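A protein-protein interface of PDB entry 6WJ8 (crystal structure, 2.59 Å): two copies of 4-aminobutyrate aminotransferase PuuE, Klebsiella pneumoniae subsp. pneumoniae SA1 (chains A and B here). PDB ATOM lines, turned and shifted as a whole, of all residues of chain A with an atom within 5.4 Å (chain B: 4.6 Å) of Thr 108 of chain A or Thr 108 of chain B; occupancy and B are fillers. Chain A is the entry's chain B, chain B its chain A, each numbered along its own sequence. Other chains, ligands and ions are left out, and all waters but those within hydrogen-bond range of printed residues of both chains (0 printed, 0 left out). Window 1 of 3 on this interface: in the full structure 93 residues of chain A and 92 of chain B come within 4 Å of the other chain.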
ATOM      1  N   PHE A 106     -34.781 -18.178  -0.677  1.00  0.00           N
ATOM      2  CA  PHE A 106     -33.516 -18.852  -0.923  1.00  0.00           C
ATOM      3  C   PHE A 106     -33.472 -19.408  -2.337  1.00  0.00           C
ATOM      4  O   PHE A 106     -34.466 -19.947  -2.837  1.00  0.00           O
ATOM      5  CB  PHE A 106     -33.287 -19.976   0.090  1.00  0.00           C
ATOM      6  CG  PHE A 106     -33.013 -19.485   1.480  1.00  0.00           C
ATOM      7  CD1 PHE A 106     -31.867 -18.756   1.756  1.00  0.00           C
ATOM      8  CD2 PHE A 106     -33.904 -19.741   2.508  1.00  0.00           C
ATOM      9  CE1 PHE A 106     -31.613 -18.297   3.035  1.00  0.00           C
ATOM     10  CE2 PHE A 106     -33.655 -19.286   3.787  1.00  0.00           C
ATOM     11  CZ  PHE A 106     -32.509 -18.561   4.049  1.00  0.00           C
ATOM     12  N   PHE A 107     -32.316 -19.270  -2.976  1.00  0.00           N
ATOM     13  CA  PHE A 107     -32.094 -19.796  -4.315  1.00  0.00           C
ATOM     14  C   PHE A 107     -30.773 -20.562  -4.274  1.00  0.00           C
ATOM     15  O   PHE A 107     -30.318 -21.019  -3.217  1.00  0.00           O
ATOM     16  CB  PHE A 107     -32.155 -18.654  -5.339  1.00  0.00           C
ATOM     17  CG  PHE A 107     -33.421 -17.847  -5.252  1.00  0.00           C
ATOM     18  CD1 PHE A 107     -34.568 -18.259  -5.913  1.00  0.00           C
ATOM     19  CD2 PHE A 107     -33.475 -16.696  -4.482  1.00  0.00           C
ATOM     20  CE1 PHE A 107     -35.740 -17.528  -5.821  1.00  0.00           C
ATOM     21  CE2 PHE A 107     -34.644 -15.960  -4.387  1.00  0.00           C
ATOM     22  CZ  PHE A 107     -35.778 -16.378  -5.055  1.00  0.00           C
ATOM     23  N   THR A 108     -30.130 -20.720  -5.427  1.00  0.00           N
ATOM     24  CA  THR A 108     -28.943 -21.562  -5.512  1.00  0.00           C
ATOM     25  C   THR A 108     -27.655 -20.785  -5.743  1.00  0.00           C
ATOM     26  O   THR A 108     -26.685 -20.977  -5.005  1.00  0.00           O
ATOM     27  CB  THR A 108     -29.117 -22.613  -6.618  1.00  0.00           C
ATOM     28  OG1 THR A 108     -30.422 -23.198  -6.522  1.00  0.00           O
ATOM     29  CG2 THR A 108     -28.077 -23.706  -6.468  1.00  0.00           C
ATOM     30  N   THR A 109     -27.610 -19.911  -6.745  1.00  0.00           N
ATOM     31  CA  THR A 109     -26.381 -19.221  -7.108  1.00  0.00           C
ATOM     32  C   THR A 109     -26.516 -17.721  -6.880  1.00  0.00           C
ATOM     33  O   THR A 109     -27.618 -17.167  -6.868  1.00  0.00           O
ATOM     34  CB  THR A 109     -26.003 -19.485  -8.570  1.00  0.00           C
ATOM     35  OG1 THR A 109     -26.942 -18.831  -9.434  1.00  0.00           O
ATOM     36  CG2 THR A 109     -26.003 -20.978  -8.857  1.00  0.00           C
ATOM     37  N   GLY A 110     -25.363 -17.070  -6.702  1.00  0.00           N
ATOM     38  CA  GLY A 110     -25.360 -15.635  -6.471  1.00  0.00           C
ATOM     39  C   GLY A 110     -25.948 -14.853  -7.628  1.00  0.00           C
ATOM     40  O   GLY A 110     -26.595 -13.821  -7.428  1.00  0.00           O
ATOM     41  N   GLU A 112     -28.350 -16.031  -9.480  1.00  0.00           N
ATOM     42  CA  GLU A 112     -29.779 -16.218  -9.259  1.00  0.00           C
ATOM     43  C   GLU A 112     -30.286 -15.297  -8.157  1.00  0.00           C
ATOM     44  O   GLU A 112     -31.414 -14.795  -8.227  1.00  0.00           O
ATOM     45  CB  GLU A 112     -30.073 -17.678  -8.911  1.00  0.00           C
ATOM     46  CG  GLU A 112     -30.232 -18.593 -10.111  1.00  0.00           C
ATOM     47  CD  GLU A 112     -30.847 -19.929  -9.741  1.00  0.00           C
ATOM     48  OE1 GLU A 112     -30.864 -20.263  -8.537  1.00  0.00           O
ATOM     49  OE2 GLU A 112     -31.314 -20.643 -10.653  1.00  0.00           O
ATOM     50  N   PRO A 274     -23.818 -25.120  -2.494  1.00  0.00           N
ATOM     51  CA  PRO A 274     -24.584 -24.237  -3.389  1.00  0.00           C
ATOM     52  C   PRO A 274     -25.838 -23.662  -2.748  1.00  0.00           C
ATOM     53  O   PRO A 274     -26.855 -24.352  -2.632  1.00  0.00           O
ATOM     54  CB  PRO A 274     -24.936 -25.153  -4.572  1.00  0.00           C
ATOM     55  CG  PRO A 274     -24.052 -26.362  -4.426  1.00  0.00           C
ATOM     56  CD  PRO A 274     -23.830 -26.515  -2.961  1.00  0.00           C
ATOM     57  N   LEU A 275     -25.781 -22.394  -2.343  1.00  0.00           N
ATOM     58  CA  LEU A 275     -26.939 -21.715  -1.779  1.00  0.00           C
ATOM     59  C   LEU A 275     -26.801 -20.215  -1.991  1.00  0.00           C
ATOM     60  O   LEU A 275     -25.696 -19.669  -1.935  1.00  0.00           O
ATOM     61  CB  LEU A 275     -27.102 -22.017  -0.285  1.00  0.00           C
ATOM     62  CG  LEU A 275     -28.397 -21.519   0.364  1.00  0.00           C
ATOM     63  CD1 LEU A 275     -29.590 -22.326  -0.127  1.00  0.00           C
ATOM     64  CD2 LEU A 275     -28.299 -21.566   1.881  1.00  0.00           C
ATOM     65  N   SER A 276     -27.932 -19.560  -2.240  1.00  0.00           N
ATOM     66  CA  SER A 276     -27.993 -18.110  -2.330  1.00  0.00           C
ATOM     67  C   SER A 276     -29.331 -17.655  -1.770  1.00  0.00           C
ATOM     68  O   SER A 276     -30.244 -18.457  -1.563  1.00  0.00           O
ATOM     69  CB  SER A 276     -27.804 -17.623  -3.767  1.00  0.00           C
ATOM     70  OG  SER A 276     -28.824 -18.123  -4.613  1.00  0.00           O
ATOM     71  N   TYR A 297     -33.422 -26.295  -7.793  1.00  0.00           N
ATOM     72  CA  TYR A 297     -32.471 -26.521  -6.715  1.00  0.00           C
ATOM     73  C   TYR A 297     -32.586 -25.504  -5.587  1.00  0.00           C
ATOM     74  O   TYR A 297     -31.878 -25.644  -4.584  1.00  0.00           O
ATOM     75  CB  TYR A 297     -31.039 -26.488  -7.258  1.00  0.00           C
ATOM     76  CG  TYR A 297     -30.685 -27.617  -8.198  1.00  0.00           C
ATOM     77  CD1 TYR A 297     -31.158 -28.906  -7.985  1.00  0.00           C
ATOM     78  CD2 TYR A 297     -29.866 -27.394  -9.297  1.00  0.00           C
ATOM     79  CE1 TYR A 297     -30.825 -29.938  -8.844  1.00  0.00           C
ATOM     80  CE2 TYR A 297     -29.530 -28.416 -10.159  1.00  0.00           C
ATOM     81  CZ  TYR A 297     -30.009 -29.685  -9.929  1.00  0.00           C
ATOM     82  OH  TYR A 297     -29.672 -30.703 -10.791  1.00  0.00           O
ATOM     83  N   ALA A 298     -33.450 -24.497  -5.726  1.00  0.00           N
ATOM     84  CA  ALA A 298     -33.482 -23.372  -4.796  1.00  0.00           C
ATOM     85  C   ALA A 298     -33.654 -23.840  -3.358  1.00  0.00           C
ATOM     86  O   ALA A 298     -34.567 -24.609  -3.043  1.00  0.00           O
ATOM     87  CB  ALA A 298     -34.610 -22.411  -5.174  1.00  0.00           C
ATOM     88  N   GLY A 299     -32.767 -23.367  -2.487  1.00  0.00           N
ATOM     89  CA  GLY A 299     -32.784 -23.756  -1.092  1.00  0.00           C
ATOM     90  C   GLY A 299     -32.358 -25.171  -0.769  1.00  0.00           C
ATOM     91  O   GLY A 299     -32.995 -25.842   0.048  1.00  0.00           O
ATOM     92  N   PHE B 107     -22.210 -26.377 -14.828  1.00  0.00           N
ATOM     93  CA  PHE B 107     -22.673 -25.229 -14.059  1.00  0.00           C
ATOM     94  C   PHE B 107     -23.552 -25.777 -12.939  1.00  0.00           C
ATOM     95  O   PHE B 107     -23.480 -26.961 -12.593  1.00  0.00           O
ATOM     96  CB  PHE B 107     -23.363 -24.216 -14.986  1.00  0.00           C
ATOM     97  CG  PHE B 107     -22.519 -23.815 -16.165  1.00  0.00           C
ATOM     98  CD1 PHE B 107     -21.586 -22.796 -16.053  1.00  0.00           C
ATOM     99  CD2 PHE B 107     -22.639 -24.474 -17.379  1.00  0.00           C
ATOM    100  CE1 PHE B 107     -20.799 -22.432 -17.132  1.00  0.00           C
ATOM    101  CE2 PHE B 107     -21.855 -24.115 -18.461  1.00  0.00           C
ATOM    102  CZ  PHE B 107     -20.932 -23.095 -18.336  1.00  0.00           C
ATOM    103  N   THR B 108     -24.395 -24.928 -12.357  1.00  0.00           N
ATOM    104  CA  THR B 108     -25.133 -25.305 -11.157  1.00  0.00           C
ATOM    105  C   THR B 108     -26.617 -25.537 -11.398  1.00  0.00           C
ATOM    106  O   THR B 108     -27.130 -26.610 -11.065  1.00  0.00           O
ATOM    107  CB  THR B 108     -24.942 -24.240 -10.070  1.00  0.00           C
ATOM    108  OG1 THR B 108     -23.543 -23.967  -9.911  1.00  0.00           O
ATOM    109  CG2 THR B 108     -25.499 -24.735  -8.748  1.00  0.00           C
ATOM    110  N   THR B 109     -27.332 -24.566 -11.960  1.00  0.00           N
ATOM    111  CA  THR B 109     -28.772 -24.674 -12.138  1.00  0.00           C
ATOM    112  C   THR B 109     -29.125 -24.880 -13.606  1.00  0.00           C
ATOM    113  O   THR B 109     -28.347 -24.563 -14.509  1.00  0.00           O
ATOM    114  CB  THR B 109     -29.491 -23.429 -11.608  1.00  0.00           C
ATOM    115  OG1 THR B 109     -29.260 -22.328 -12.496  1.00  0.00           O
ATOM    116  CG2 THR B 109     -28.986 -23.073 -10.220  1.00  0.00           C
ATOM    117  N   GLY B 110     -30.327 -25.418 -13.828  1.00  0.00           N
ATOM    118  CA  GLY B 110     -30.788 -25.640 -15.189  1.00  0.00           C
ATOM    119  C   GLY B 110     -30.903 -24.355 -15.985  1.00  0.00           C
ATOM    120  O   GLY B 110     -30.561 -24.314 -17.169  1.00  0.00           O
ATOM    121  N   GLU B 112     -29.049 -21.794 -15.520  1.00  0.00           N
ATOM    122  CA  GLU B 112     -27.668 -21.444 -15.838  1.00  0.00           C
ATOM    123  C   GLU B 112     -27.168 -22.223 -17.047  1.00  0.00           C
ATOM    124  O   GLU B 112     -26.424 -21.686 -17.877  1.00  0.00           O
ATOM    125  CB  GLU B 112     -26.769 -21.702 -14.629  1.00  0.00           C
ATOM    126  CG  GLU B 112     -26.778 -20.596 -13.593  1.00  0.00           C
ATOM    127  CD  GLU B 112     -25.687 -20.768 -12.556  1.00  0.00           C
ATOM    128  OE1 GLU B 112     -25.140 -21.886 -12.448  1.00  0.00           O
ATOM    129  OE2 GLU B 112     -25.376 -19.785 -11.851  1.00  0.00           O
ATOM    130  N   PRO B 274     -27.220 -29.983  -6.603  1.00  0.00           N
ATOM    131  CA  PRO B 274     -27.162 -28.869  -7.563  1.00  0.00           C
ATOM    132  C   PRO B 274     -26.050 -29.010  -8.590  1.00  0.00           C
ATOM    133  O   PRO B 274     -24.885 -28.716  -8.303  1.00  0.00           O
ATOM    134  CB  PRO B 274     -26.938 -27.641  -6.667  1.00  0.00           C
ATOM    135  CG  PRO B 274     -27.270 -28.091  -5.276  1.00  0.00           C
ATOM    136  CD  PRO B 274     -26.926 -29.541  -5.230  1.00  0.00           C
ATOM    137  N   LEU B 275     -26.403 -29.447  -9.798  1.00  0.00           N
ATOM    138  CA  LEU B 275     -25.451 -29.548 -10.893  1.00  0.00           C
ATOM    139  C   LEU B 275     -26.191 -29.398 -12.212  1.00  0.00           C
ATOM    140  O   LEU B 275     -27.326 -29.861 -12.350  1.00  0.00           O
ATOM    141  CB  LEU B 275     -24.693 -30.880 -10.869  1.00  0.00           C
ATOM    142  CG  LEU B 275     -23.570 -31.034 -11.898  1.00  0.00           C
ATOM    143  CD1 LEU B 275     -22.289 -30.379 -11.402  1.00  0.00           C
ATOM    144  CD2 LEU B 275     -23.334 -32.498 -12.228  1.00  0.00           C
ATOM    145  N   SER B 276     -25.542 -28.747 -13.172  1.00  0.00           N
ATOM    146  CA  SER B 276     -26.070 -28.629 -14.522  1.00  0.00           C
ATOM    147  C   SER B 276     -24.903 -28.649 -15.496  1.00  0.00           C
ATOM    148  O   SER B 276     -23.743 -28.483 -15.110  1.00  0.00           O
ATOM    149  CB  SER B 276     -26.913 -27.362 -14.690  1.00  0.00           C
ATOM    150  OG  SER B 276     -26.110 -26.199 -14.592  1.00  0.00           O
ATOM    151  N   TYR B 297     -20.241 -21.618  -7.925  1.00  0.00           N
ATOM    152  CA  TYR B 297     -20.625 -22.968  -7.534  1.00  0.00           C
ATOM    153  C   TYR B 297     -20.508 -23.976  -8.668  1.00  0.00           C
ATOM    154  O   TYR B 297     -20.670 -25.176  -8.416  1.00  0.00           O
ATOM    155  CB  TYR B 297     -22.063 -22.981  -7.013  1.00  0.00           C
ATOM    156  CG  TYR B 297     -22.264 -22.251  -5.707  1.00  0.00           C
ATOM    157  CD1 TYR B 297     -21.293 -22.275  -4.715  1.00  0.00           C
ATOM    158  CD2 TYR B 297     -23.433 -21.542  -5.464  1.00  0.00           C
ATOM    159  CE1 TYR B 297     -21.480 -21.609  -3.518  1.00  0.00           C
ATOM    160  CE2 TYR B 297     -23.629 -20.875  -4.273  1.00  0.00           C
ATOM    161  CZ  TYR B 297     -22.652 -20.911  -3.303  1.00  0.00           C
ATOM    162  OH  TYR B 297     -22.847 -20.245  -2.117  1.00  0.00           O
ATOM    163  N   ALA B 298     -20.233 -23.521  -9.892  1.00  0.00           N
ATOM    164  CA  ALA B 298     -20.285 -24.376 -11.073  1.00  0.00           C
ATOM    165  C   ALA B 298     -19.486 -25.657 -10.872  1.00  0.00           C
ATOM    166  O   ALA B 298     -18.350 -25.629 -10.390  1.00  0.00           O
ATOM    167  CB  ALA B 298     -19.761 -23.616 -12.292  1.00  0.00           C
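Of the 10 printed residues of chain B, 6 touch a printed residue of chain A.
Of the 12 printed residues of chain A, 6 touch a printed residue of chain B.
Hydrophobic or aromatic side chains of chain A within 4 Å of the printed part of chain B: Pro 274 and Tyr 297.
The backbone NH (N) of Thr 108 of chain A lies within hydrogen-bond range of the side-chain carboxylate (OE1) of Glu 112 of chain A.
The side-chain hydroxyl (OG) of Ser 276 of chain B sits at hydrogen-bond distance from the backbone carbonyl oxygen (O) of Thr 109 of chain B (2.8 Å).
O of Tyr 297 of chain A sits close to OG1 of Thr 108 of chain A, at 3.4 Å.
The side-chain hydroxyl (OG) of Ser 276 of chain B sits at hydrogen-bond distance from the backbone NH (N) of Thr 108 of chain B, at 3.1 Å.
The side-chain hydroxyl (OG1) of Thr 109 of chain B lies within hydrogen-bond range of the backbone NH (N) of Glu 112 of chain B.
N of Thr 108 of chain B lies within hydrogen-bond range of OE1 of Glu 112 of chain B, 3.1 Å away.
Among the printed residues, merely in contact across the chains: Tyr 297 of chain A with Thr 108 of chain B (3.1 Å), Thr 108 of chain A with Tyr 297 of chain B (3.1 Å), Tyr 297 of chain A with Pro 274 of chain B (3.5 Å), Pro 274 of chain A with Tyr 297 of chain B (3.6 Å), Thr 108 of chain A with Thr 108 of chain B (3.6 Å), Thr 108 of chain A with Thr 109 of chain B (3.6 Å), Thr 109 of chain A with Thr 108 of chain B (3.6 Å), Pro 274 of chain A with Pro 274 of chain B (3.8 Å) and Thr 109 of chain A with Thr 109 of chain B (3.9 Å).
Thr 108 of chain B touches its own counterpart, Thr 108 of chain A.
Thr 108 of chain A touches Tyr 297 of chain B, and with the chains exchanged Tyr 297 of chain A touches Thr 108 of chain B.
Thr 109 of chain A touches its own counterpart, Thr 109 of chain B.
Pro 274 of chain A touches its own counterpart, Pro 274 of chain B.
Positions printed for both chains: 107, 108, 109, 110, 112, 274, 275, 276, 297 and 298.
Of the 13 pairs that touch across the chains among the printed residues, 13 have their exchanged pair printed and touching as well.
OE2 of Glu 112 of chain B sits at hydrogen-bond distance from OG1 of Thr 109 of chain A (3.0 Å).
The side-chain hydroxyl (OG1) of Thr 109 of chain B sits at hydrogen-bond distance from the side-chain carboxylate (OE2) of Glu 112 of chain A (3.2 Å).
The backbone carbonyl oxygen (O) of Leu 275 of chain B sits at hydrogen-bond distance from the side-chain hydroxyl (OH) of Tyr 297 of chain A (2.9 Å).
The side-chain hydroxyl of Tyr 297 of chain B is in hydrogen-bond range of the backbone carbonyl oxygen of Leu 275 of chain A.
Thr 108 of chain A touches just these residues of chain B: Thr 108, Thr 109 and Tyr 297.
Of chain A, only Thr 108 (3.6 Å), Thr 109 (3.6 Å) and Tyr 297 (3.1 Å) come within 4 Å of Thr 108 of chain B.
Of the printed residues of chain B, Glu 112 of chain A touches Thr 109 (3.2 Å).
Printed residues of chain B within 4 Å of Pro 274 of chain A: Pro 274 and Tyr 297.
Of the printed residues of chain A, Pro 274 of chain B touches Pro 274 (3.8 Å) and Tyr 297 (3.5 Å).
Gly 299 of chain A touches none of the printed residues of chain B.
Ala 298 of chain A touches none of the printed residues of chain B.
The nearest residue of chain B that does not touch Thr 108 of chain A is Pro 274 of chain B (4.1 Å).
The nearest residue of chain A that does not touch Thr 108 of chain B is Pro 274 of chain A (4.2 Å).
The nearest printed residue of chain A that does not touch Glu 112 of chain B is Glu 112 of chain A (5.3 Å).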
